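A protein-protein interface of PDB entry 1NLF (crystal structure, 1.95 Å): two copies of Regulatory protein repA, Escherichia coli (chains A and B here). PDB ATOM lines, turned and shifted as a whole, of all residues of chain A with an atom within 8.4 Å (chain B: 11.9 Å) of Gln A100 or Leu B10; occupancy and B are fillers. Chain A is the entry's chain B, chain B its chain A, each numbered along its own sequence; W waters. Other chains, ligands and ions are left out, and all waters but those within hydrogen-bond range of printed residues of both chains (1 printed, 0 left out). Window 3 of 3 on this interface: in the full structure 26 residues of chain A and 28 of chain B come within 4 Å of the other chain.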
ATOM      1  N   ALA A  55      34.870  13.849  -8.733  1.00  0.00           N
ATOM      2  CA  ALA A  55      34.611  15.283  -8.630  1.00  0.00           C
ATOM      3  C   ALA A  55      33.671  15.591  -7.471  1.00  0.00           C
ATOM      4  O   ALA A  55      33.628  16.722  -6.990  1.00  0.00           O
ATOM      5  CB  ALA A  55      34.021  15.812  -9.942  1.00  0.00           C
ATOM      6  N   GLY A  56      32.923  14.585  -7.025  1.00  0.00           N
ATOM      7  CA  GLY A  56      32.001  14.783  -5.918  1.00  0.00           C
ATOM      8  C   GLY A  56      30.624  14.187  -6.161  1.00  0.00           C
ATOM      9  O   GLY A  56      29.742  14.272  -5.308  1.00  0.00           O
ATOM     10  N   GLY A  57      30.436  13.582  -7.328  1.00  0.00           N
ATOM     11  CA  GLY A  57      29.157  12.978  -7.653  1.00  0.00           C
ATOM     12  C   GLY A  57      28.964  11.633  -6.971  1.00  0.00           C
ATOM     13  O   GLY A  57      29.857  11.166  -6.271  1.00  0.00           O
ATOM     14  N   LEU A  87      26.182  14.344 -21.293  1.00  0.00           N
ATOM     15  CA  LEU A  87      25.986  14.928 -19.969  1.00  0.00           C
ATOM     16  C   LEU A  87      24.511  14.988 -19.598  1.00  0.00           C
ATOM     17  O   LEU A  87      24.134  14.732 -18.450  1.00  0.00           O
ATOM     18  CB  LEU A  87      26.580  16.343 -19.916  1.00  0.00           C
ATOM     19  CG  LEU A  87      28.105  16.437 -19.806  1.00  0.00           C
ATOM     20  CD1 LEU A  87      28.544  17.873 -20.003  1.00  0.00           C
ATOM     21  CD2 LEU A  87      28.557  15.909 -18.446  1.00  0.00           C
ATOM     22  N   HIS A  88      23.670  15.344 -20.562  1.00  0.00           N
ATOM     23  CA  HIS A  88      22.241  15.433 -20.282  1.00  0.00           C
ATOM     24  C   HIS A  88      21.673  14.059 -19.929  1.00  0.00           C
ATOM     25  O   HIS A  88      20.792  13.941 -19.079  1.00  0.00           O
ATOM     26  CB  HIS A  88      21.482  16.006 -21.480  1.00  0.00           C
ATOM     27  CG  HIS A  88      20.052  16.325 -21.174  1.00  0.00           C
ATOM     28  ND1 HIS A  88      19.687  17.307 -20.279  1.00  0.00           N
ATOM     29  CD2 HIS A  88      18.900  15.747 -21.589  1.00  0.00           C
ATOM     30  CE1 HIS A  88      18.371  17.319 -20.153  1.00  0.00           C
ATOM     31  NE2 HIS A  88      17.869  16.382 -20.939  1.00  0.00           N
ATOM     32  N   GLY A  91      22.767  13.189 -16.485  1.00  0.00           N
ATOM     33  CA  GLY A  91      22.057  14.035 -15.538  1.00  0.00           C
ATOM     34  C   GLY A  91      20.753  13.455 -15.007  1.00  0.00           C
ATOM     35  O   GLY A  91      20.334  13.768 -13.892  1.00  0.00           O
ATOM     36  N   LEU A  94      21.102  11.887 -11.684  1.00  0.00           N
ATOM     37  CA  LEU A  94      21.591  12.714 -10.588  1.00  0.00           C
ATOM     38  C   LEU A  94      20.554  13.675 -10.021  1.00  0.00           C
ATOM     39  O   LEU A  94      19.764  14.271 -10.755  1.00  0.00           O
ATOM     40  CB  LEU A  94      22.821  13.516 -11.037  1.00  0.00           C
ATOM     41  CG  LEU A  94      24.149  12.775 -11.246  1.00  0.00           C
ATOM     42  CD1 LEU A  94      23.994  11.687 -12.287  1.00  0.00           C
ATOM     43  CD2 LEU A  94      25.209  13.769 -11.685  1.00  0.00           C
ATOM     44  N   SER A  95      20.567  13.820  -8.702  1.00  0.00           N
ATOM     45  CA  SER A  95      19.650  14.725  -8.029  1.00  0.00           C
ATOM     46  C   SER A  95      20.184  16.140  -8.224  1.00  0.00           C
ATOM     47  O   SER A  95      21.309  16.329  -8.690  1.00  0.00           O
ATOM     48  CB  SER A  95      19.590  14.404  -6.537  1.00  0.00           C
ATOM     49  OG  SER A  95      20.840  14.662  -5.928  1.00  0.00           O
ATOM     50  N   ALA A  96      19.380  17.131  -7.862  1.00  0.00           N
ATOM     51  CA  ALA A  96      19.785  18.520  -8.006  1.00  0.00           C
ATOM     52  C   ALA A  96      21.106  18.767  -7.285  1.00  0.00           C
ATOM     53  O   ALA A  96      22.016  19.384  -7.834  1.00  0.00           O
ATOM     54  CB  ALA A  96      18.702  19.436  -7.446  1.00  0.00           C
ATOM     55  N   GLU A  97      21.211  18.262  -6.061  1.00  0.00           N
ATOM     56  CA  GLU A  97      22.414  18.444  -5.249  1.00  0.00           C
ATOM     57  C   GLU A  97      23.637  17.758  -5.863  1.00  0.00           C
ATOM     58  O   GLU A  97      24.745  18.297  -5.832  1.00  0.00           O
ATOM     59  CB  GLU A  97      22.165  17.906  -3.834  1.00  0.00           C
ATOM     60  CG  GLU A  97      23.023  18.543  -2.743  1.00  0.00           C
ATOM     61  CD  GLU A  97      24.460  18.056  -2.740  1.00  0.00           C
ATOM     62  OE1 GLU A  97      25.268  18.602  -1.958  1.00  0.00           O
ATOM     63  OE2 GLU A  97      24.783  17.125  -3.508  1.00  0.00           O
ATOM     64  N   GLU A  98      23.430  16.569  -6.420  1.00  0.00           N
ATOM     65  CA  GLU A  98      24.518  15.816  -7.036  1.00  0.00           C
ATOM     66  C   GLU A  98      24.986  16.489  -8.324  1.00  0.00           C
ATOM     67  O   GLU A  98      26.173  16.498  -8.628  1.00  0.00           O
ATOM     68  CB  GLU A  98      24.061  14.382  -7.318  1.00  0.00           C
ATOM     69  CG  GLU A  98      23.580  13.661  -6.063  1.00  0.00           C
ATOM     70  CD  GLU A  98      22.992  12.295  -6.349  1.00  0.00           C
ATOM     71  OE1 GLU A  98      22.250  12.163  -7.342  1.00  0.00           O
ATOM     72  OE2 GLU A  98      23.263  11.358  -5.571  1.00  0.00           O
ATOM     73  N   ARG A  99      24.049  17.052  -9.081  1.00  0.00           N
ATOM     74  CA  ARG A  99      24.403  17.738 -10.319  1.00  0.00           C
ATOM     75  C   ARG A  99      25.330  18.903 -10.001  1.00  0.00           C
ATOM     76  O   ARG A  99      26.332  19.123 -10.685  1.00  0.00           O
ATOM     77  CB  ARG A  99      23.150  18.265 -11.023  1.00  0.00           C
ATOM     78  CG  ARG A  99      22.299  17.183 -11.670  1.00  0.00           C
ATOM     79  CD  ARG A  99      21.065  17.780 -12.334  1.00  0.00           C
ATOM     80  NE  ARG A  99      20.228  16.755 -12.949  1.00  0.00           N
ATOM     81  CZ  ARG A  99      19.104  17.004 -13.617  1.00  0.00           C
ATOM     82  NH1 ARG A  99      18.675  18.252 -13.765  1.00  0.00           N
ATOM     83  NH2 ARG A  99      18.400  16.003 -14.130  1.00  0.00           N
ATOM     84  N   GLN A 100      24.989  19.640  -8.946  1.00  0.00           N
ATOM     85  CA  GLN A 100      25.773  20.791  -8.523  1.00  0.00           C
ATOM     86  C   GLN A 100      27.152  20.364  -8.028  1.00  0.00           C
ATOM     87  O   GLN A 100      28.153  21.041  -8.277  1.00  0.00           O
ATOM     88  CB  GLN A 100      25.036  21.545  -7.412  1.00  0.00           C
ATOM     89  CG  GLN A 100      25.715  22.832  -6.992  1.00  0.00           C
ATOM     90  CD  GLN A 100      25.645  23.897  -8.066  1.00  0.00           C
ATOM     91  OE1 GLN A 100      24.559  24.321  -8.461  1.00  0.00           O
ATOM     92  NE2 GLN A 100      26.805  24.336  -8.547  1.00  0.00           N
ATOM     93  N   ALA A 101      27.205  19.244  -7.322  1.00  0.00           N
ATOM     94  CA  ALA A 101      28.476  18.754  -6.815  1.00  0.00           C
ATOM     95  C   ALA A 101      29.385  18.444  -7.995  1.00  0.00           C
ATOM     96  O   ALA A 101      30.563  18.796  -7.987  1.00  0.00           O
ATOM     97  CB  ALA A 101      28.262  17.504  -5.968  1.00  0.00           C
ATOM     98  N   VAL A 102      28.830  17.788  -9.011  1.00  0.00           N
ATOM     99  CA  VAL A 102      29.603  17.431 -10.197  1.00  0.00           C
ATOM    100  C   VAL A 102      30.070  18.682 -10.930  1.00  0.00           C
ATOM    101  O   VAL A 102      31.238  18.797 -11.302  1.00  0.00           O
ATOM    102  CB  VAL A 102      28.783  16.551 -11.166  1.00  0.00           C
ATOM    103  CG1 VAL A 102      29.559  16.341 -12.463  1.00  0.00           C
ATOM    104  CG2 VAL A 102      28.487  15.201 -10.524  1.00  0.00           C
ATOM    105  N   ALA A 103      29.157  19.626 -11.138  1.00  0.00           N
ATOM    106  CA  ALA A 103      29.505  20.865 -11.822  1.00  0.00           C
ATOM    107  C   ALA A 103      30.577  21.636 -11.047  1.00  0.00           C
ATOM    108  O   ALA A 103      31.429  22.296 -11.647  1.00  0.00           O
ATOM    109  CB  ALA A 103      28.261  21.732 -12.007  1.00  0.00           C
ATOM    110  N   ASP A 104      30.543  21.547  -9.719  1.00  0.00           N
ATOM    111  CA  ASP A 104      31.527  22.244  -8.893  1.00  0.00           C
ATOM    112  C   ASP A 104      32.923  21.621  -8.950  1.00  0.00           C
ATOM    113  O   ASP A 104      33.926  22.324  -8.832  1.00  0.00           O
ATOM    114  CB  ASP A 104      31.086  22.288  -7.423  1.00  0.00           C
ATOM    115  CG  ASP A 104      29.932  23.245  -7.176  1.00  0.00           C
ATOM    116  OD1 ASP A 104      29.749  24.190  -7.970  1.00  0.00           O
ATOM    117  OD2 ASP A 104      29.213  23.060  -6.170  1.00  0.00           O
ATOM    118  N   GLY A 105      32.992  20.307  -9.129  1.00  0.00           N
ATOM    119  CA  GLY A 105      34.289  19.653  -9.144  1.00  0.00           C
ATOM    120  C   GLY A 105      34.830  19.152 -10.470  1.00  0.00           C
ATOM    121  O   GLY A 105      35.970  18.694 -10.525  1.00  0.00           O
ATOM    122  N   LEU A 106      34.043  19.245 -11.537  1.00  0.00           N
ATOM    123  CA  LEU A 106      34.499  18.761 -12.838  1.00  0.00           C
ATOM    124  C   LEU A 106      34.612  19.832 -13.919  1.00  0.00           C
ATOM    125  O   LEU A 106      33.700  20.634 -14.108  1.00  0.00           O
ATOM    126  CB  LEU A 106      33.565  17.649 -13.323  1.00  0.00           C
ATOM    127  CG  LEU A 106      33.762  17.064 -14.726  1.00  0.00           C
ATOM    128  CD1 LEU A 106      35.151  16.463 -14.870  1.00  0.00           C
ATOM    129  CD2 LEU A 106      32.702  16.003 -14.960  1.00  0.00           C
ATOM    130  N   LYS B   5      35.621  26.712 -25.579  1.00  0.00           N
ATOM    131  CA  LYS B   5      35.401  27.186 -24.224  1.00  0.00           C
ATOM    132  C   LYS B   5      34.965  25.973 -23.406  1.00  0.00           C
ATOM    133  O   LYS B   5      34.414  25.014 -23.951  1.00  0.00           O
ATOM    134  CB  LYS B   5      34.324  28.276 -24.197  1.00  0.00           C
ATOM    135  CG  LYS B   5      33.008  27.894 -24.848  1.00  0.00           C
ATOM    136  CD  LYS B   5      32.073  29.093 -24.915  1.00  0.00           C
ATOM    137  CE  LYS B   5      30.794  28.765 -25.668  1.00  0.00           C
ATOM    138  NZ  LYS B   5      29.903  29.954 -25.790  1.00  0.00           N
ATOM    139  N   PRO B   6      35.235  25.983 -22.092  1.00  0.00           N
ATOM    140  CA  PRO B   6      34.844  24.852 -21.244  1.00  0.00           C
ATOM    141  C   PRO B   6      33.337  24.610 -21.346  1.00  0.00           C
ATOM    142  O   PRO B   6      32.569  25.544 -21.581  1.00  0.00           O
ATOM    143  CB  PRO B   6      35.258  25.311 -19.847  1.00  0.00           C
ATOM    144  CG  PRO B   6      36.423  26.219 -20.122  1.00  0.00           C
ATOM    145  CD  PRO B   6      35.939  27.011 -21.307  1.00  0.00           C
ATOM    146  N   ILE B   7      32.918  23.362 -21.165  1.00  0.00           N
ATOM    147  CA  ILE B   7      31.496  23.016 -21.232  1.00  0.00           C
ATOM    148  C   ILE B   7      30.763  23.532 -20.000  1.00  0.00           C
ATOM    149  O   ILE B   7      31.278  23.442 -18.888  1.00  0.00           O
ATOM    150  CB  ILE B   7      31.278  21.478 -21.274  1.00  0.00           C
ATOM    151  CG1 ILE B   7      31.877  20.877 -22.554  1.00  0.00           C
ATOM    152  CG2 ILE B   7      29.786  21.161 -21.158  1.00  0.00           C
ATOM    153  CD1 ILE B   7      31.169  21.263 -23.828  1.00  0.00           C
ATOM    154  N   ASN B   8      29.567  24.083 -20.201  1.00  0.00           N
ATOM    155  CA  ASN B   8      28.763  24.556 -19.077  1.00  0.00           C
ATOM    156  C   ASN B   8      28.019  23.308 -18.598  1.00  0.00           C
ATOM    157  O   ASN B   8      26.969  22.951 -19.136  1.00  0.00           O
ATOM    158  CB  ASN B   8      27.758  25.615 -19.533  1.00  0.00           C
ATOM    159  CG  ASN B   8      27.009  26.249 -18.369  1.00  0.00           C
ATOM    160  OD1 ASN B   8      26.611  25.568 -17.422  1.00  0.00           O
ATOM    161  ND2 ASN B   8      26.800  27.559 -18.445  1.00  0.00           N
ATOM    162  N   ILE B   9      28.574  22.642 -17.593  1.00  0.00           N
ATOM    163  CA  ILE B   9      27.986  21.415 -17.075  1.00  0.00           C
ATOM    164  C   ILE B   9      26.566  21.509 -16.534  1.00  0.00           C
ATOM    165  O   ILE B   9      25.704  20.699 -16.895  1.00  0.00           O
ATOM    166  CB  ILE B   9      28.875  20.800 -15.972  1.00  0.00           C
ATOM    167  CG1 ILE B   9      30.281  20.566 -16.520  1.00  0.00           C
ATOM    168  CG2 ILE B   9      28.256  19.507 -15.456  1.00  0.00           C
ATOM    169  CD1 ILE B   9      30.318  19.926 -17.883  1.00  0.00           C
ATOM    170  N   LEU B  10      26.323  22.477 -15.658  1.00  0.00           N
ATOM    171  CA  LEU B  10      25.000  22.630 -15.071  1.00  0.00           C
ATOM    172  C   LEU B  10      23.936  22.836 -16.147  1.00  0.00           C
ATOM    173  O   LEU B  10      22.842  22.282 -16.063  1.00  0.00           O
ATOM    174  CB  LEU B  10      24.997  23.798 -14.080  1.00  0.00           C
ATOM    175  CG  LEU B  10      24.012  23.645 -12.921  1.00  0.00           C
ATOM    176  CD1 LEU B  10      24.205  22.277 -12.254  1.00  0.00           C
ATOM    177  CD2 LEU B  10      24.227  24.771 -11.919  1.00  0.00           C
ATOM    178  N   GLU B  11      24.268  23.616 -17.168  1.00  0.00           N
ATOM    179  CA  GLU B  11      23.340  23.885 -18.260  1.00  0.00           C
ATOM    180  C   GLU B  11      23.014  22.613 -19.043  1.00  0.00           C
ATOM    181  O   GLU B  11      21.859  22.379 -19.402  1.00  0.00           O
ATOM    182  CB  GLU B  11      23.937  24.950 -19.192  1.00  0.00           C
ATOM    183  CG  GLU B  11      23.268  25.055 -20.552  1.00  0.00           C
ATOM    184  CD  GLU B  11      23.929  26.091 -21.441  1.00  0.00           C
ATOM    185  OE1 GLU B  11      23.675  27.296 -21.233  1.00  0.00           O
ATOM    186  OE2 GLU B  11      24.713  25.701 -22.335  1.00  0.00           O
ATOM    187  N   ALA B  12      24.031  21.795 -19.303  1.00  0.00           N
ATOM    188  CA  ALA B  12      23.848  20.546 -20.035  1.00  0.00           C
ATOM    189  C   ALA B  12      22.911  19.598 -19.283  1.00  0.00           C
ATOM    190  O   ALA B  12      22.124  18.873 -19.896  1.00  0.00           O
ATOM    191  CB  ALA B  12      25.200  19.874 -20.268  1.00  0.00           C
ATOM    192  N   PHE B  13      23.010  19.602 -17.955  1.00  0.00           N
ATOM    193  CA  PHE B  13      22.169  18.764 -17.095  1.00  0.00           C
ATOM    194  C   PHE B  13      20.725  19.276 -17.067  1.00  0.00           C
ATOM    195  O   PHE B  13      19.776  18.526 -17.286  1.00  0.00           O
ATOM    196  CB  PHE B  13      22.672  18.800 -15.644  1.00  0.00           C
ATOM    197  CG  PHE B  13      23.921  17.998 -15.381  1.00  0.00           C
ATOM    198  CD1 PHE B  13      24.720  18.300 -14.275  1.00  0.00           C
ATOM    199  CD2 PHE B  13      24.272  16.916 -16.186  1.00  0.00           C
ATOM    200  CE1 PHE B  13      25.850  17.535 -13.972  1.00  0.00           C
ATOM    201  CE2 PHE B  13      25.394  16.144 -15.895  1.00  0.00           C
ATOM    202  CZ  PHE B  13      26.187  16.452 -14.785  1.00  0.00           C
ATOM    203  N   ALA B  14      20.584  20.567 -16.787  1.00  0.00           N
ATOM    204  CA  ALA B  14      19.279  21.212 -16.647  1.00  0.00           C
ATOM    205  C   ALA B  14      18.342  21.274 -17.851  1.00  0.00           C
ATOM    206  O   ALA B  14      17.125  21.238 -17.682  1.00  0.00           O
ATOM    207  CB  ALA B  14      19.474  22.617 -16.083  1.00  0.00           C
ATOM    208  N   ALA B  15      18.883  21.377 -19.058  1.00  0.00           N
ATOM    209  CA  ALA B  15      18.028  21.467 -20.238  1.00  0.00           C
ATOM    210  C   ALA B  15      18.488  20.556 -21.364  1.00  0.00           C
ATOM    211  O   ALA B  15      19.681  20.292 -21.506  1.00  0.00           O
ATOM    212  CB  ALA B  15      17.975  22.911 -20.726  1.00  0.00           C
ATOM    213  N   ALA B  16      17.533  20.076 -22.157  1.00  0.00           N
ATOM    214  CA  ALA B  16      17.840  19.197 -23.280  1.00  0.00           C
ATOM    215  C   ALA B  16      18.580  19.979 -24.362  1.00  0.00           C
ATOM    216  O   ALA B  16      18.081  20.989 -24.864  1.00  0.00           O
ATOM    217  CB  ALA B  16      16.553  18.598 -23.851  1.00  0.00           C
ATOM    218  N   PRO B  17      19.791  19.530 -24.727  1.00  0.00           N
ATOM    219  CA  PRO B  17      20.574  20.217 -25.759  1.00  0.00           C
ATOM    220  C   PRO B  17      19.913  20.059 -27.124  1.00  0.00           C
ATOM    221  O   PRO B  17      19.173  19.104 -27.354  1.00  0.00           O
ATOM    222  CB  PRO B  17      21.928  19.503 -25.709  1.00  0.00           C
ATOM    223  CG  PRO B  17      21.984  18.938 -24.320  1.00  0.00           C
ATOM    224  CD  PRO B  17      20.580  18.452 -24.105  1.00  0.00           C
HETATM  225  O   HOH W   1      19.981  15.741 -17.146  1.00  0.00           O
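NH2 of Arg A99 lies within hydrogen-bond range of O of Gly A91, 3.0 Å away.
The backbone carbonyl oxygen (O) of Leu A94 sits at hydrogen-bond distance from the guanidinium group (NE) of Arg A99, 3.3 Å away.
The side-chain carboxylate (OD1) of Asp A104 lies within hydrogen-bond range of the side-chain amide nitrogen (NE2) of Gln A100 (3.0 Å).
Of the 13 printed residues of chain B, 8 touch a printed residue of chain A.
Hydrophobic or aromatic side chains of chain B that line the printed part of chain A: Ile B7, Ile B9, Leu B10, Ala B12, Phe B13, Ala B16 and Pro B17.
Hydrophobic or aromatic side chains of chain A within 4 Å of the printed part of chain B: Leu A87 and His A88.
Among the printed residues, 12 pairs touch across the chains.
Among the printed residues, no Asp or Glu carboxylate lies within 4 Å of a Lys or Arg side-chain nitrogen of the other chain.
ND1 of His A88 sits at hydrogen-bond distance from O of Ala B12.
The backbone carbonyl oxygen (O) of Phe B13 lies within hydrogen-bond range of a ring nitrogen (ND1) of His A88 (3.2 Å).
The backbone carbonyl oxygen (O) of Ala B15 sits at hydrogen-bond distance from a ring nitrogen (ND1) of His A88 (3.2 Å).
No residue of chain B comes within 4 Å of Ala A96.
No residue of chain B comes within 4 Å of Glu A97.
Of chain B, only Leu B10 (3.5 Å) comes within 4 Å of Gln A100.
No residue of chain B comes within 4 Å of Ala A101.
No residue of chain B comes within 4 Å of Val A102.
Of the printed residues of chain A, Ile B7 touches Leu A87 (3.7 Å).
Of chain A, only Gln A100 (3.5 Å) comes within 4 Å of Leu B10.
Of the printed residues of chain A, Ala B16 touches His A88 (3.5 Å).
The nearest residue of chain B that does not touch Gln A100 is Phe B13 (5.5 Å).
The nearest printed residue of chain A that does not touch Leu B10 is Ala A103 (4.1 Å).
The nearest printed residue of chain A that does not touch Ala B15 is Arg A99 (6.2 Å).
Water W1 lies within hydrogen-bond range of the backbone carbonyl oxygen (O) of His A88 (2.8 Å), the backbone carbonyl oxygen (O) of Phe B13 (2.8 Å) and the guanidinium group (NH2) of Arg A99 (3.4 Å).
No position is printed for both chains.
Among the printed residues, merely in contact across the chains: Leu A87 with Ile B7, Leu A87 with Ile B9, Leu A87 with Ala B12, Leu A87 with Phe B13, His A88 with Ala B16, His A88 with Pro B17, Gly A91 with Phe B13, Arg A99 with Phe B13 and Gln A100 with Leu B10.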
